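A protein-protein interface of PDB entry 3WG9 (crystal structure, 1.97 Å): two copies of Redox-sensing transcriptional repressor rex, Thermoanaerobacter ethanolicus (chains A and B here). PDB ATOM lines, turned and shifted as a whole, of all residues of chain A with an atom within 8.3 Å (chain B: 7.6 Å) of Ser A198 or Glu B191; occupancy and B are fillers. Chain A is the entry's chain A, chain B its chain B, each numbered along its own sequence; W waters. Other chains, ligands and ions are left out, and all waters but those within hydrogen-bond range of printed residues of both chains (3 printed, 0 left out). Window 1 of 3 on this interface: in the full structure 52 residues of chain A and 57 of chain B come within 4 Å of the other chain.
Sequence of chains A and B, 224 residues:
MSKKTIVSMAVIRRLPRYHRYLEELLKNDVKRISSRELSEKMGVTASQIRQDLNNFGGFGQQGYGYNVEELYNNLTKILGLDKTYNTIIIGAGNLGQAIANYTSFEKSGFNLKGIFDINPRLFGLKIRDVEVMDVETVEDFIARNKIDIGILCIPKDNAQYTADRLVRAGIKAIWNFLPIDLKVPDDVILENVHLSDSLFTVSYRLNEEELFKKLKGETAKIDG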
ATOM      1  N   HIS A 194      -2.472   4.907  -6.733  1.00  0.00           N
ATOM      2  CA  HIS A 194      -2.565   3.644  -7.438  1.00  0.00           C
ATOM      3  C   HIS A 194      -3.678   2.817  -6.767  1.00  0.00           C
ATOM      4  O   HIS A 194      -3.373   2.002  -5.887  1.00  0.00           O
ATOM      5  CB  HIS A 194      -1.236   2.851  -7.295  1.00  0.00           C
ATOM      6  CG  HIS A 194      -0.011   3.623  -7.742  1.00  0.00           C
ATOM      7  ND1 HIS A 194       0.197   3.963  -9.059  1.00  0.00           N
ATOM      8  CD2 HIS A 194       1.026   4.151  -7.044  1.00  0.00           C
ATOM      9  CE1 HIS A 194       1.299   4.686  -9.158  1.00  0.00           C
ATOM     10  NE2 HIS A 194       1.860   4.756  -7.957  1.00  0.00           N
ATOM     11  N   LEU A 195      -4.929   2.993  -7.216  1.00  0.00           N
ATOM     12  CA  LEU A 195      -6.045   2.241  -6.669  1.00  0.00           C
ATOM     13  C   LEU A 195      -5.913   0.750  -6.869  1.00  0.00           C
ATOM     14  O   LEU A 195      -6.394   0.032  -6.026  1.00  0.00           O
ATOM     15  CB  LEU A 195      -7.413   2.642  -7.238  1.00  0.00           C
ATOM     16  CG  LEU A 195      -7.797   4.118  -6.995  1.00  0.00           C
ATOM     17  CD1 LEU A 195      -9.176   4.376  -7.576  1.00  0.00           C
ATOM     18  CD2 LEU A 195      -7.725   4.509  -5.518  1.00  0.00           C
ATOM     19  N   SER A 196      -5.260   0.255  -7.928  1.00  0.00           N
ATOM     20  CA  SER A 196      -5.183  -1.202  -8.064  1.00  0.00           C
ATOM     21  C   SER A 196      -4.339  -1.835  -6.930  1.00  0.00           C
ATOM     22  O   SER A 196      -4.502  -3.050  -6.660  1.00  0.00           O
ATOM     23  CB  SER A 196      -4.631  -1.641  -9.431  1.00  0.00           C
ATOM     24  OG  SER A 196      -3.365  -1.042  -9.632  1.00  0.00           O
ATOM     25  N   ASP A 197      -3.428  -1.081  -6.320  1.00  0.00           N
ATOM     26  CA  ASP A 197      -2.591  -1.656  -5.264  1.00  0.00           C
ATOM     27  C   ASP A 197      -3.556  -2.136  -4.154  1.00  0.00           C
ATOM     28  O   ASP A 197      -3.262  -3.109  -3.477  1.00  0.00           O
ATOM     29  CB  ASP A 197      -1.630  -0.668  -4.668  1.00  0.00           C
ATOM     30  CG  ASP A 197      -0.370  -0.412  -5.547  1.00  0.00           C
ATOM     31  OD1 ASP A 197      -0.245  -0.990  -6.651  1.00  0.00           O
ATOM     32  OD2 ASP A 197       0.449   0.404  -5.064  1.00  0.00           O
ATOM     33  N   SER A 198      -4.666  -1.414  -3.940  1.00  0.00           N
ATOM     34  CA  SER A 198      -5.666  -1.812  -2.947  1.00  0.00           C
ATOM     35  C   SER A 198      -6.552  -2.933  -3.554  1.00  0.00           C
ATOM     36  O   SER A 198      -6.806  -3.972  -2.894  1.00  0.00           O
ATOM     37  CB  SER A 198      -6.516  -0.538  -2.571  1.00  0.00           C
ATOM     38  OG  SER A 198      -7.635  -0.842  -1.758  1.00  0.00           O
ATOM     39  N   LEU A 199      -7.097  -2.720  -4.747  1.00  0.00           N
ATOM     40  CA  LEU A 199      -8.042  -3.747  -5.274  1.00  0.00           C
ATOM     41  C   LEU A 199      -7.404  -5.134  -5.373  1.00  0.00           C
ATOM     42  O   LEU A 199      -8.054  -6.146  -5.100  1.00  0.00           O
ATOM     43  CB  LEU A 199      -8.511  -3.339  -6.666  1.00  0.00           C
ATOM     44  CG  LEU A 199      -9.523  -4.237  -7.363  1.00  0.00           C
ATOM     45  CD1 LEU A 199     -10.744  -4.341  -6.496  1.00  0.00           C
ATOM     46  CD2 LEU A 199      -9.787  -3.687  -8.792  1.00  0.00           C
ATOM     47  N   PHE A 200      -6.112  -5.163  -5.749  1.00  0.00           N
ATOM     48  CA  PHE A 200      -5.488  -6.452  -6.022  1.00  0.00           C
ATOM     49  C   PHE A 200      -5.187  -7.180  -4.682  1.00  0.00           C
ATOM     50  O   PHE A 200      -4.923  -8.374  -4.703  1.00  0.00           O
ATOM     51  CB  PHE A 200      -4.212  -6.333  -6.874  1.00  0.00           C
ATOM     52  CG  PHE A 200      -4.465  -5.874  -8.325  1.00  0.00           C
ATOM     53  CD1 PHE A 200      -5.745  -5.822  -8.851  1.00  0.00           C
ATOM     54  CD2 PHE A 200      -3.394  -5.500  -9.131  1.00  0.00           C
ATOM     55  CE1 PHE A 200      -5.953  -5.400 -10.181  1.00  0.00           C
ATOM     56  CE2 PHE A 200      -3.587  -5.079 -10.443  1.00  0.00           C
ATOM     57  CZ  PHE A 200      -4.886  -5.012 -10.942  1.00  0.00           C
ATOM     58  N   THR A 201      -5.259  -6.493  -3.541  1.00  0.00           N
ATOM     59  CA  THR A 201      -5.232  -7.231  -2.263  1.00  0.00           C
ATOM     60  C   THR A 201      -6.550  -7.982  -1.987  1.00  0.00           C
ATOM     61  O   THR A 201      -6.625  -8.975  -1.220  1.00  0.00           O
ATOM     62  CB  THR A 201      -4.846  -6.398  -1.050  1.00  0.00           C
ATOM     63  OG1 THR A 201      -5.966  -5.589  -0.688  1.00  0.00           O
ATOM     64  CG2 THR A 201      -3.542  -5.498  -1.268  1.00  0.00           C
ATOM     65  N   VAL A 202      -7.604  -7.535  -2.624  1.00  0.00           N
ATOM     66  CA  VAL A 202      -8.887  -8.216  -2.485  1.00  0.00           C
ATOM     67  C   VAL A 202      -8.926  -9.477  -3.331  1.00  0.00           C
ATOM     68  O   VAL A 202      -9.351 -10.546  -2.839  1.00  0.00           O
ATOM     69  CB  VAL A 202     -10.052  -7.290  -2.889  1.00  0.00           C
ATOM     70  CG1 VAL A 202     -11.427  -8.058  -2.763  1.00  0.00           C
ATOM     71  CG2 VAL A 202     -10.047  -6.060  -1.998  1.00  0.00           C
ATOM     72  N   SER A 203      -8.525  -9.376  -4.594  1.00  0.00           N
ATOM     73  CA  SER A 203      -8.411 -10.613  -5.369  1.00  0.00           C
ATOM     74  C   SER A 203      -7.436 -11.568  -4.688  1.00  0.00           C
ATOM     75  O   SER A 203      -7.662 -12.783  -4.683  1.00  0.00           O
ATOM     76  CB  SER A 203      -7.964 -10.353  -6.795  1.00  0.00           C
ATOM     77  OG  SER A 203      -6.945  -9.370  -6.838  1.00  0.00           O
ATOM     78  N   TYR A 204      -6.359 -11.016  -4.124  1.00  0.00           N
ATOM     79  CA  TYR A 204      -5.343 -11.902  -3.506  1.00  0.00           C
ATOM     80  C   TYR A 204      -6.060 -12.684  -2.390  1.00  0.00           C
ATOM     81  O   TYR A 204      -6.014 -13.924  -2.313  1.00  0.00           O
ATOM     82  CB  TYR A 204      -4.174 -11.097  -2.880  1.00  0.00           C
ATOM     83  CG  TYR A 204      -3.317 -12.098  -2.102  1.00  0.00           C
ATOM     84  CD1 TYR A 204      -3.582 -12.399  -0.773  1.00  0.00           C
ATOM     85  CD2 TYR A 204      -2.340 -12.829  -2.743  1.00  0.00           C
ATOM     86  CE1 TYR A 204      -2.866 -13.398  -0.075  1.00  0.00           C
ATOM     87  CE2 TYR A 204      -1.583 -13.800  -2.038  1.00  0.00           C
ATOM     88  CZ  TYR A 204      -1.879 -14.083  -0.701  1.00  0.00           C
ATOM     89  OH  TYR A 204      -1.210 -15.042   0.032  1.00  0.00           O
ATOM     90  N   ARG A 205      -6.791 -11.963  -1.549  1.00  0.00           N
ATOM     91  CA  ARG A 205      -7.428 -12.607  -0.402  1.00  0.00           C
ATOM     92  C   ARG A 205      -8.535 -13.570  -0.772  1.00  0.00           C
ATOM     93  O   ARG A 205      -8.630 -14.629  -0.169  1.00  0.00           O
ATOM     94  CB  ARG A 205      -7.862 -11.577   0.647  1.00  0.00           C
ATOM     95  CG  ARG A 205      -6.628 -11.046   1.411  1.00  0.00           C
ATOM     96  CD  ARG A 205      -7.056  -9.922   2.365  1.00  0.00           C
ATOM     97  NE  ARG A 205      -7.165  -8.634   1.684  1.00  0.00           N
ATOM     98  CZ  ARG A 205      -7.513  -7.514   2.309  1.00  0.00           C
ATOM     99  NH1 ARG A 205      -7.794  -7.554   3.632  1.00  0.00           N
ATOM    100  NH2 ARG A 205      -7.485  -6.358   1.656  1.00  0.00           N
ATOM    101  N   MET B   9      -0.421  -9.463   5.990  1.00  0.00           N
ATOM    102  CA  MET B   9      -0.905  -8.341   5.201  1.00  0.00           C
ATOM    103  C   MET B   9       0.287  -7.430   4.755  1.00  0.00           C
ATOM    104  O   MET B   9       0.257  -6.832   3.688  1.00  0.00           O
ATOM    105  CB  MET B   9      -1.927  -7.531   6.015  1.00  0.00           C
ATOM    106  CG  MET B   9      -3.355  -8.125   5.983  1.00  0.00           C
ATOM    107  SD  MET B   9      -3.992  -8.214   4.278  1.00  0.00           S
ATOM    108  CE  MET B   9      -4.092  -6.529   3.704  1.00  0.00           C
ATOM    109  N   ILE B  12       1.319  -9.104   1.682  1.00  0.00           N
ATOM    110  CA  ILE B  12       0.272  -9.026   0.615  1.00  0.00           C
ATOM    111  C   ILE B  12       0.263  -7.622   0.029  1.00  0.00           C
ATOM    112  O   ILE B  12       0.107  -7.459  -1.162  1.00  0.00           O
ATOM    113  CB  ILE B  12      -1.094  -9.382   1.209  1.00  0.00           C
ATOM    114  CG1 ILE B  12      -1.115 -10.870   1.555  1.00  0.00           C
ATOM    115  CG2 ILE B  12      -2.336  -8.984   0.239  1.00  0.00           C
ATOM    116  CD1 ILE B  12      -2.371 -11.225   2.488  1.00  0.00           C
ATOM    117  N   ARG B  13       0.454  -6.587   0.843  1.00  0.00           N
ATOM    118  CA  ARG B  13       0.418  -5.223   0.292  1.00  0.00           C
ATOM    119  C   ARG B  13       1.654  -4.843  -0.518  1.00  0.00           C
ATOM    120  O   ARG B  13       1.592  -3.938  -1.333  1.00  0.00           O
ATOM    121  CB  ARG B  13       0.259  -4.154   1.393  1.00  0.00           C
ATOM    122  CG  ARG B  13      -1.144  -4.285   2.097  1.00  0.00           C
ATOM    123  CD  ARG B  13      -1.578  -2.994   2.789  1.00  0.00           C
ATOM    124  NE  ARG B  13      -2.868  -3.169   3.462  1.00  0.00           N
ATOM    125  CZ  ARG B  13      -4.046  -3.076   2.829  1.00  0.00           C
ATOM    126  NH1 ARG B  13      -4.119  -2.860   1.499  1.00  0.00           N
ATOM    127  NH2 ARG B  13      -5.154  -3.143   3.543  1.00  0.00           N
ATOM    128  N   PRO B  16       1.205  -6.283  -4.942  1.00  0.00           N
ATOM    129  CA  PRO B  16       0.776  -5.460  -6.084  1.00  0.00           C
ATOM    130  C   PRO B  16       1.803  -4.413  -6.516  1.00  0.00           C
ATOM    131  O   PRO B  16       1.817  -4.074  -7.693  1.00  0.00           O
ATOM    132  CB  PRO B  16      -0.550  -4.818  -5.619  1.00  0.00           C
ATOM    133  CG  PRO B  16      -0.980  -5.748  -4.429  1.00  0.00           C
ATOM    134  CD  PRO B  16       0.325  -6.115  -3.783  1.00  0.00           C
ATOM    135  N   TYR B 102     -13.015   3.220 -13.738  1.00  0.00           N
ATOM    136  CA  TYR B 102     -11.694   2.660 -13.408  1.00  0.00           C
ATOM    137  C   TYR B 102     -11.657   1.112 -13.543  1.00  0.00           C
ATOM    138  O   TYR B 102     -10.711   0.535 -14.093  1.00  0.00           O
ATOM    139  CB  TYR B 102     -11.290   3.094 -11.983  1.00  0.00           C
ATOM    140  CG  TYR B 102      -9.924   2.615 -11.571  1.00  0.00           C
ATOM    141  CD1 TYR B 102      -8.805   3.385 -11.864  1.00  0.00           C
ATOM    142  CD2 TYR B 102      -9.742   1.385 -10.876  1.00  0.00           C
ATOM    143  CE1 TYR B 102      -7.500   2.930 -11.535  1.00  0.00           C
ATOM    144  CE2 TYR B 102      -8.444   0.933 -10.510  1.00  0.00           C
ATOM    145  CZ  TYR B 102      -7.329   1.726 -10.860  1.00  0.00           C
ATOM    146  OH  TYR B 102      -6.023   1.384 -10.549  1.00  0.00           O
ATOM    147  N   GLY B 150     -18.575  -6.251  -3.169  1.00  0.00           N
ATOM    148  CA  GLY B 150     -19.472  -5.058  -3.157  1.00  0.00           C
ATOM    149  C   GLY B 150     -18.550  -3.838  -2.959  1.00  0.00           C
ATOM    150  O   GLY B 150     -17.709  -3.780  -2.047  1.00  0.00           O
ATOM    151  N   LEU B 152     -18.266   0.103  -2.110  1.00  0.00           N
ATOM    152  CA  LEU B 152     -19.115   1.064  -1.438  1.00  0.00           C
ATOM    153  C   LEU B 152     -18.690   2.468  -1.809  1.00  0.00           C
ATOM    154  O   LEU B 152     -17.535   2.859  -1.517  1.00  0.00           O
ATOM    155  CB  LEU B 152     -19.114   0.925   0.105  1.00  0.00           C
ATOM    156  CG  LEU B 152     -19.574  -0.364   0.790  1.00  0.00           C
ATOM    157  CD1 LEU B 152     -19.430  -0.161   2.324  1.00  0.00           C
ATOM    158  CD2 LEU B 152     -21.027  -0.717   0.440  1.00  0.00           C
ATOM    159  N   ALA B 173     -16.540  -9.996  -0.109  1.00  0.00           N
ATOM    160  CA  ALA B 173     -15.594  -8.910   0.140  1.00  0.00           C
ATOM    161  C   ALA B 173     -16.292  -7.594  -0.136  1.00  0.00           C
ATOM    162  O   ALA B 173     -17.188  -7.520  -1.024  1.00  0.00           O
ATOM    163  CB  ALA B 173     -14.472  -9.026  -0.888  1.00  0.00           C
ATOM    164  N   ILE B 174     -15.790  -6.569   0.551  1.00  0.00           N
ATOM    165  CA  ILE B 174     -16.236  -5.213   0.389  1.00  0.00           C
ATOM    166  C   ILE B 174     -15.035  -4.336   0.170  1.00  0.00           C
ATOM    167  O   ILE B 174     -14.030  -4.390   0.930  1.00  0.00           O
ATOM    168  CB  ILE B 174     -17.001  -4.738   1.673  1.00  0.00           C
ATOM    169  CG1 ILE B 174     -18.366  -5.477   1.690  1.00  0.00           C
ATOM    170  CG2 ILE B 174     -17.219  -3.205   1.616  1.00  0.00           C
ATOM    171  CD1 ILE B 174     -19.187  -5.207   2.969  1.00  0.00           C
ATOM    172  N   TRP B 175     -15.120  -3.539  -0.896  1.00  0.00           N
ATOM    173  CA  TRP B 175     -14.071  -2.534  -1.171  1.00  0.00           C
ATOM    174  C   TRP B 175     -14.673  -1.176  -0.808  1.00  0.00           C
ATOM    175  O   TRP B 175     -15.620  -0.693  -1.439  1.00  0.00           O
ATOM    176  CB  TRP B 175     -13.652  -2.629  -2.653  1.00  0.00           C
ATOM    177  CG  TRP B 175     -12.362  -1.944  -2.991  1.00  0.00           C
ATOM    178  CD1 TRP B 175     -11.278  -1.774  -2.157  1.00  0.00           C
ATOM    179  CD2 TRP B 175     -11.991  -1.386  -4.246  1.00  0.00           C
ATOM    180  NE1 TRP B 175     -10.229  -1.167  -2.839  1.00  0.00           N
ATOM    181  CE2 TRP B 175     -10.656  -0.891  -4.117  1.00  0.00           C
ATOM    182  CE3 TRP B 175     -12.630  -1.285  -5.479  1.00  0.00           C
ATOM    183  CZ2 TRP B 175     -10.005  -0.224  -5.141  1.00  0.00           C
ATOM    184  CZ3 TRP B 175     -11.962  -0.630  -6.527  1.00  0.00           C
ATOM    185  CH2 TRP B 175     -10.634  -0.170  -6.365  1.00  0.00           C
ATOM    186  N   ASN B 176     -14.188  -0.586   0.279  1.00  0.00           N
ATOM    187  CA  ASN B 176     -14.916   0.512   0.926  1.00  0.00           C
ATOM    188  C   ASN B 176     -14.212   1.858   0.630  1.00  0.00           C
ATOM    189  O   ASN B 176     -13.121   2.047   1.110  1.00  0.00           O
ATOM    190  CB  ASN B 176     -14.917   0.296   2.448  1.00  0.00           C
ATOM    191  CG  ASN B 176     -15.509   1.485   3.215  1.00  0.00           C
ATOM    192  OD1 ASN B 176     -16.405   2.192   2.717  1.00  0.00           O
ATOM    193  ND2 ASN B 176     -14.949   1.756   4.402  1.00  0.00           N
ATOM    194  N   PHE B 177     -14.827   2.752  -0.136  1.00  0.00           N
ATOM    195  CA  PHE B 177     -14.244   4.091  -0.403  1.00  0.00           C
ATOM    196  C   PHE B 177     -14.592   5.185   0.613  1.00  0.00           C
ATOM    197  O   PHE B 177     -14.135   6.325   0.475  1.00  0.00           O
ATOM    198  CB  PHE B 177     -14.660   4.590  -1.769  1.00  0.00           C
ATOM    199  CG  PHE B 177     -13.871   3.952  -2.865  1.00  0.00           C
ATOM    200  CD1 PHE B 177     -12.705   4.566  -3.324  1.00  0.00           C
ATOM    201  CD2 PHE B 177     -14.199   2.673  -3.279  1.00  0.00           C
ATOM    202  CE1 PHE B 177     -11.924   3.973  -4.312  1.00  0.00           C
ATOM    203  CE2 PHE B 177     -13.431   2.062  -4.279  1.00  0.00           C
ATOM    204  CZ  PHE B 177     -12.288   2.699  -4.762  1.00  0.00           C
ATOM    205  N   LEU B 178     -15.439   4.859   1.575  1.00  0.00           N
ATOM    206  CA  LEU B 178     -15.839   5.868   2.538  1.00  0.00           C
ATOM    207  C   LEU B 178     -14.800   5.996   3.609  1.00  0.00           C
ATOM    208  O   LEU B 178     -14.304   4.981   4.098  1.00  0.00           O
ATOM    209  CB  LEU B 178     -17.164   5.554   3.205  1.00  0.00           C
ATOM    210  CG  LEU B 178     -18.310   4.699   2.666  1.00  0.00           C
ATOM    211  CD1 LEU B 178     -19.575   5.288   3.308  1.00  0.00           C
ATOM    212  CD2 LEU B 178     -18.453   4.547   1.151  1.00  0.00           C
ATOM    213  N   ASP B 181     -14.112   3.295   8.917  1.00  0.00           N
ATOM    214  CA  ASP B 181     -13.823   1.871   9.013  1.00  0.00           C
ATOM    215  C   ASP B 181     -15.027   1.008   9.477  1.00  0.00           C
ATOM    216  O   ASP B 181     -15.414   0.999  10.661  1.00  0.00           O
ATOM    217  CB  ASP B 181     -12.545   1.633   9.825  1.00  0.00           C
ATOM    218  CG  ASP B 181     -11.272   2.044   9.055  1.00  0.00           C
ATOM    219  OD1 ASP B 181     -11.355   2.744   8.011  1.00  0.00           O
ATOM    220  OD2 ASP B 181     -10.167   1.637   9.467  1.00  0.00           O
ATOM    221  N   LEU B 182     -15.589   0.273   8.510  1.00  0.00           N
ATOM    222  CA  LEU B 182     -16.809  -0.543   8.687  1.00  0.00           C
ATOM    223  C   LEU B 182     -16.602  -1.809   9.524  1.00  0.00           C
ATOM    224  O   LEU B 182     -15.492  -2.282   9.623  1.00  0.00           O
ATOM    225  CB  LEU B 182     -17.372  -0.930   7.321  1.00  0.00           C
ATOM    226  CG  LEU B 182     -17.737   0.274   6.462  1.00  0.00           C
ATOM    227  CD1 LEU B 182     -18.191  -0.245   5.132  1.00  0.00           C
ATOM    228  CD2 LEU B 182     -18.804   1.158   7.090  1.00  0.00           C
ATOM    229  N   VAL B 184     -17.440  -5.799   9.750  1.00  0.00           N
ATOM    230  CA  VAL B 184     -17.931  -7.000   9.038  1.00  0.00           C
ATOM    231  C   VAL B 184     -17.412  -8.209   9.811  1.00  0.00           C
ATOM    232  O   VAL B 184     -16.429  -8.107  10.556  1.00  0.00           O
ATOM    233  CB  VAL B 184     -17.381  -7.089   7.558  1.00  0.00           C
ATOM    234  CG1 VAL B 184     -17.846  -5.852   6.693  1.00  0.00           C
ATOM    235  CG2 VAL B 184     -15.915  -7.145   7.571  1.00  0.00           C
ATOM    236  N   VAL B 188     -15.400 -12.157   6.130  1.00  0.00           N
ATOM    237  CA  VAL B 188     -15.652 -11.278   4.997  1.00  0.00           C
ATOM    238  C   VAL B 188     -14.400 -10.421   4.814  1.00  0.00           C
ATOM    239  O   VAL B 188     -13.874  -9.863   5.778  1.00  0.00           O
ATOM    240  CB  VAL B 188     -16.871 -10.347   5.276  1.00  0.00           C
ATOM    241  CG1 VAL B 188     -17.094  -9.302   4.120  1.00  0.00           C
ATOM    242  CG2 VAL B 188     -18.164 -11.234   5.450  1.00  0.00           C
ATOM    243  N   ILE B 189     -13.906 -10.314   3.594  1.00  0.00           N
ATOM    244  CA  ILE B 189     -12.724  -9.461   3.343  1.00  0.00           C
ATOM    245  C   ILE B 189     -13.176  -8.003   3.341  1.00  0.00           C
ATOM    246  O   ILE B 189     -14.126  -7.685   2.634  1.00  0.00           O
ATOM    247  CB  ILE B 189     -12.069  -9.792   1.991  1.00  0.00           C
ATOM    248  CG1 ILE B 189     -11.471 -11.200   2.036  1.00  0.00           C
ATOM    249  CG2 ILE B 189     -10.889  -8.818   1.686  1.00  0.00           C
ATOM    250  CD1 ILE B 189     -11.502 -11.959   0.669  1.00  0.00           C
ATOM    251  N   LEU B 190     -12.544  -7.123   4.134  1.00  0.00           N
ATOM    252  CA  LEU B 190     -12.933  -5.705   4.073  1.00  0.00           C
ATOM    253  C   LEU B 190     -11.697  -4.903   3.741  1.00  0.00           C
ATOM    254  O   LEU B 190     -10.725  -4.982   4.480  1.00  0.00           O
ATOM    255  CB  LEU B 190     -13.484  -5.178   5.402  1.00  0.00           C
ATOM    256  CG  LEU B 190     -13.655  -3.636   5.525  1.00  0.00           C
ATOM    257  CD1 LEU B 190     -14.653  -2.998   4.483  1.00  0.00           C
ATOM    258  CD2 LEU B 190     -14.126  -3.295   6.926  1.00  0.00           C
ATOM    259  N   GLU B 191     -11.687  -4.218   2.599  1.00  0.00           N
ATOM    260  CA  GLU B 191     -10.500  -3.420   2.236  1.00  0.00           C
ATOM    261  C   GLU B 191     -10.936  -1.948   2.228  1.00  0.00           C
ATOM    262  O   GLU B 191     -11.793  -1.553   1.409  1.00  0.00           O
ATOM    263  CB  GLU B 191     -10.000  -3.850   0.836  1.00  0.00           C
ATOM    264  CG  GLU B 191      -8.953  -2.908   0.174  1.00  0.00           C
ATOM    265  CD  GLU B 191      -7.610  -2.850   0.941  1.00  0.00           C
ATOM    266  OE1 GLU B 191      -7.446  -3.551   1.975  1.00  0.00           O
ATOM    267  OE2 GLU B 191      -6.739  -2.052   0.490  1.00  0.00           O
ATOM    268  N   ASN B 192     -10.447  -1.190   3.218  1.00  0.00           N
ATOM    269  CA  ASN B 192     -10.768   0.228   3.330  1.00  0.00           C
ATOM    270  C   ASN B 192      -9.780   1.015   2.519  1.00  0.00           C
ATOM    271  O   ASN B 192      -8.532   0.875   2.642  1.00  0.00           O
ATOM    272  CB  ASN B 192     -10.823   0.763   4.784  1.00  0.00           C
ATOM    273  CG  ASN B 192     -11.799   0.015   5.675  1.00  0.00           C
ATOM    274  OD1 ASN B 192     -13.014  -0.036   5.426  1.00  0.00           O
ATOM    275  ND2 ASN B 192     -11.269  -0.563   6.746  1.00  0.00           N
ATOM    276  N   VAL B 193     -10.329   1.810   1.606  1.00  0.00           N
ATOM    277  CA  VAL B 193      -9.455   2.675   0.856  1.00  0.00           C
ATOM    278  C   VAL B 193      -9.273   3.881   1.764  1.00  0.00           C
ATOM    279  O   VAL B 193     -10.228   4.544   2.219  1.00  0.00           O
ATOM    280  CB  VAL B 193     -10.079   3.109  -0.514  1.00  0.00           C
ATOM    281  CG1 VAL B 193      -9.135   3.980  -1.289  1.00  0.00           C
ATOM    282  CG2 VAL B 193     -10.417   1.889  -1.442  1.00  0.00           C
ATOM    283  N   HIS B 194      -8.039   4.269   1.878  1.00  0.00           N
ATOM    284  CA  HIS B 194      -7.664   5.345   2.766  1.00  0.00           C
ATOM    285  C   HIS B 194      -6.917   6.299   1.832  1.00  0.00           C
ATOM    286  O   HIS B 194      -5.735   6.382   1.909  1.00  0.00           O
ATOM    287  CB  HIS B 194      -6.669   4.740   3.801  1.00  0.00           C
ATOM    288  CG  HIS B 194      -7.323   3.798   4.795  1.00  0.00           C
ATOM    289  ND1 HIS B 194      -8.384   4.175   5.590  1.00  0.00           N
ATOM    290  CD2 HIS B 194      -7.011   2.523   5.157  1.00  0.00           C
ATOM    291  CE1 HIS B 194      -8.736   3.164   6.360  1.00  0.00           C
ATOM    292  NE2 HIS B 194      -7.928   2.146   6.107  1.00  0.00           N
HETATM  293  O   HOH W   1      -2.449  -2.091  -0.476  1.00  0.00           O
HETATM  294  O   HOH W   2      -1.134  -2.708  -8.489  1.00  0.00           O
HETATM  295  O   HOH W   3      -7.960  -4.989   4.843  1.00  0.00           O
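Leu A195 touches Trp B175. Asp A197 touches Pro B16 (O to CG, 3.6 Å). Ser A198 touches Val B193. CG2 of Thr A201 touches NH1 of Arg B13, at 3.9 Å. Val A202 touches Ala B173. Glu B191 touches Val A202. Tyr A204 touches Ile B12. Arg A205 touches Met B9 (CZ to CE, 3.8 Å). Ile B189 touches Arg A205. Arg A205 touches Leu B190.
Water W2 lies within hydrogen-bond range of the side-chain carboxylate (OD1) of Asp A197 (2.7 Å), the side-chain hydroxyl (OG) of Ser A196 (3.0 Å) and the backbone carbonyl oxygen (O) of Pro B16 (3.3 Å). Water W1 bridges the guanidinium group (NH1) of Arg B13 and the backbone carbonyl oxygen (O) of Asp A197. Water W3 lies within hydrogen-bond range of the backbone carbonyl oxygen (O) of Leu B190 (2.8 Å), the guanidinium group (NH1) of Arg A205 (2.8 Å) and the side-chain carboxylate (OE1) of Glu B191 (3.2 Å).
Of chain A, only Ser A198, Thr A201, Val A202 and Arg A205 come within 4 Å of Glu B191. Printed residues of chain A within 4 Å of Met B9: Arg A205. Of the printed residues of chain B, Asp A197 touches Pro B16 (3.6 Å). Of the printed residues of chain A, Pro B16 touches Asp A197. Asp B181 touches none of the printed residues of chain A. The nearest printed residue of chain B that does not touch Ser A198 is Asn B192 (4.8 Å). The nearest printed residue of chain B that does not touch Tyr A204 is Ile B189 (6.3 Å).
N of Ser A196 sits at hydrogen-bond distance from OH of Tyr B102 (3.0 Å). The side-chain hydroxyl of Ser A198 is in hydrogen-bond range of the indole nitrogen of Trp B175 (2.8 Å). OE2 of Glu B191 lies within hydrogen-bond range of OG of Ser A198, at 2.7 Å. The side-chain carboxylate (OE1) of Glu B191 lies within salt-bridge range of the guanidinium group (NH2) of Arg A205 (2.8 Å).
NH2 of Arg B13 lies within salt-bridge range of OE1 of Glu B191 (2.8 Å). The backbone carbonyl oxygen (O) of Gly B150 lies within hydrogen-bond range of the backbone NH (N) of Trp B175 (2.8 Å). The backbone NH of Leu B152 is in hydrogen-bond range of the backbone carbonyl oxygen of Trp B175 (2.8 Å). O of Ile B189 is in hydrogen-bond range of N of Ile B174 (2.9 Å). The backbone NH (N) of Glu B191 is in hydrogen-bond range of the backbone carbonyl oxygen (O) of Ile B174, at 2.9 Å. The backbone NH of Val B193 is in hydrogen-bond range of the backbone carbonyl oxygen of Asn B176 (2.8 Å).
1 position is printed for both chains. Of the 18 pairs that touch across the chains among the printed residues, none has its exchanged pair printed and touching as well.
Of the 23 printed residues of chain B, 11 touch a printed residue of chain A. Printed residues of chain B that touch a printed residue of chain A: Met B9, Ile B12, Arg B13, Pro B16, Tyr B102, Ala B173, Trp B175, Ile B189, Leu B190, Glu B191 and Val B193. Hydrophobic or aromatic side chains of chain B that line the printed part of chain A: Met B9, Ile B12, Pro B16, Tyr B102, Ala B173, Trp B175, Ile B189 and Val B193. Among the printed residues, 18 pairs touch across the chains. Among the printed residues, Asp or Glu carboxylates within 4 Å of a Lys or Arg side-chain nitrogen of the other chain: Arg A205 with Glu B191.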
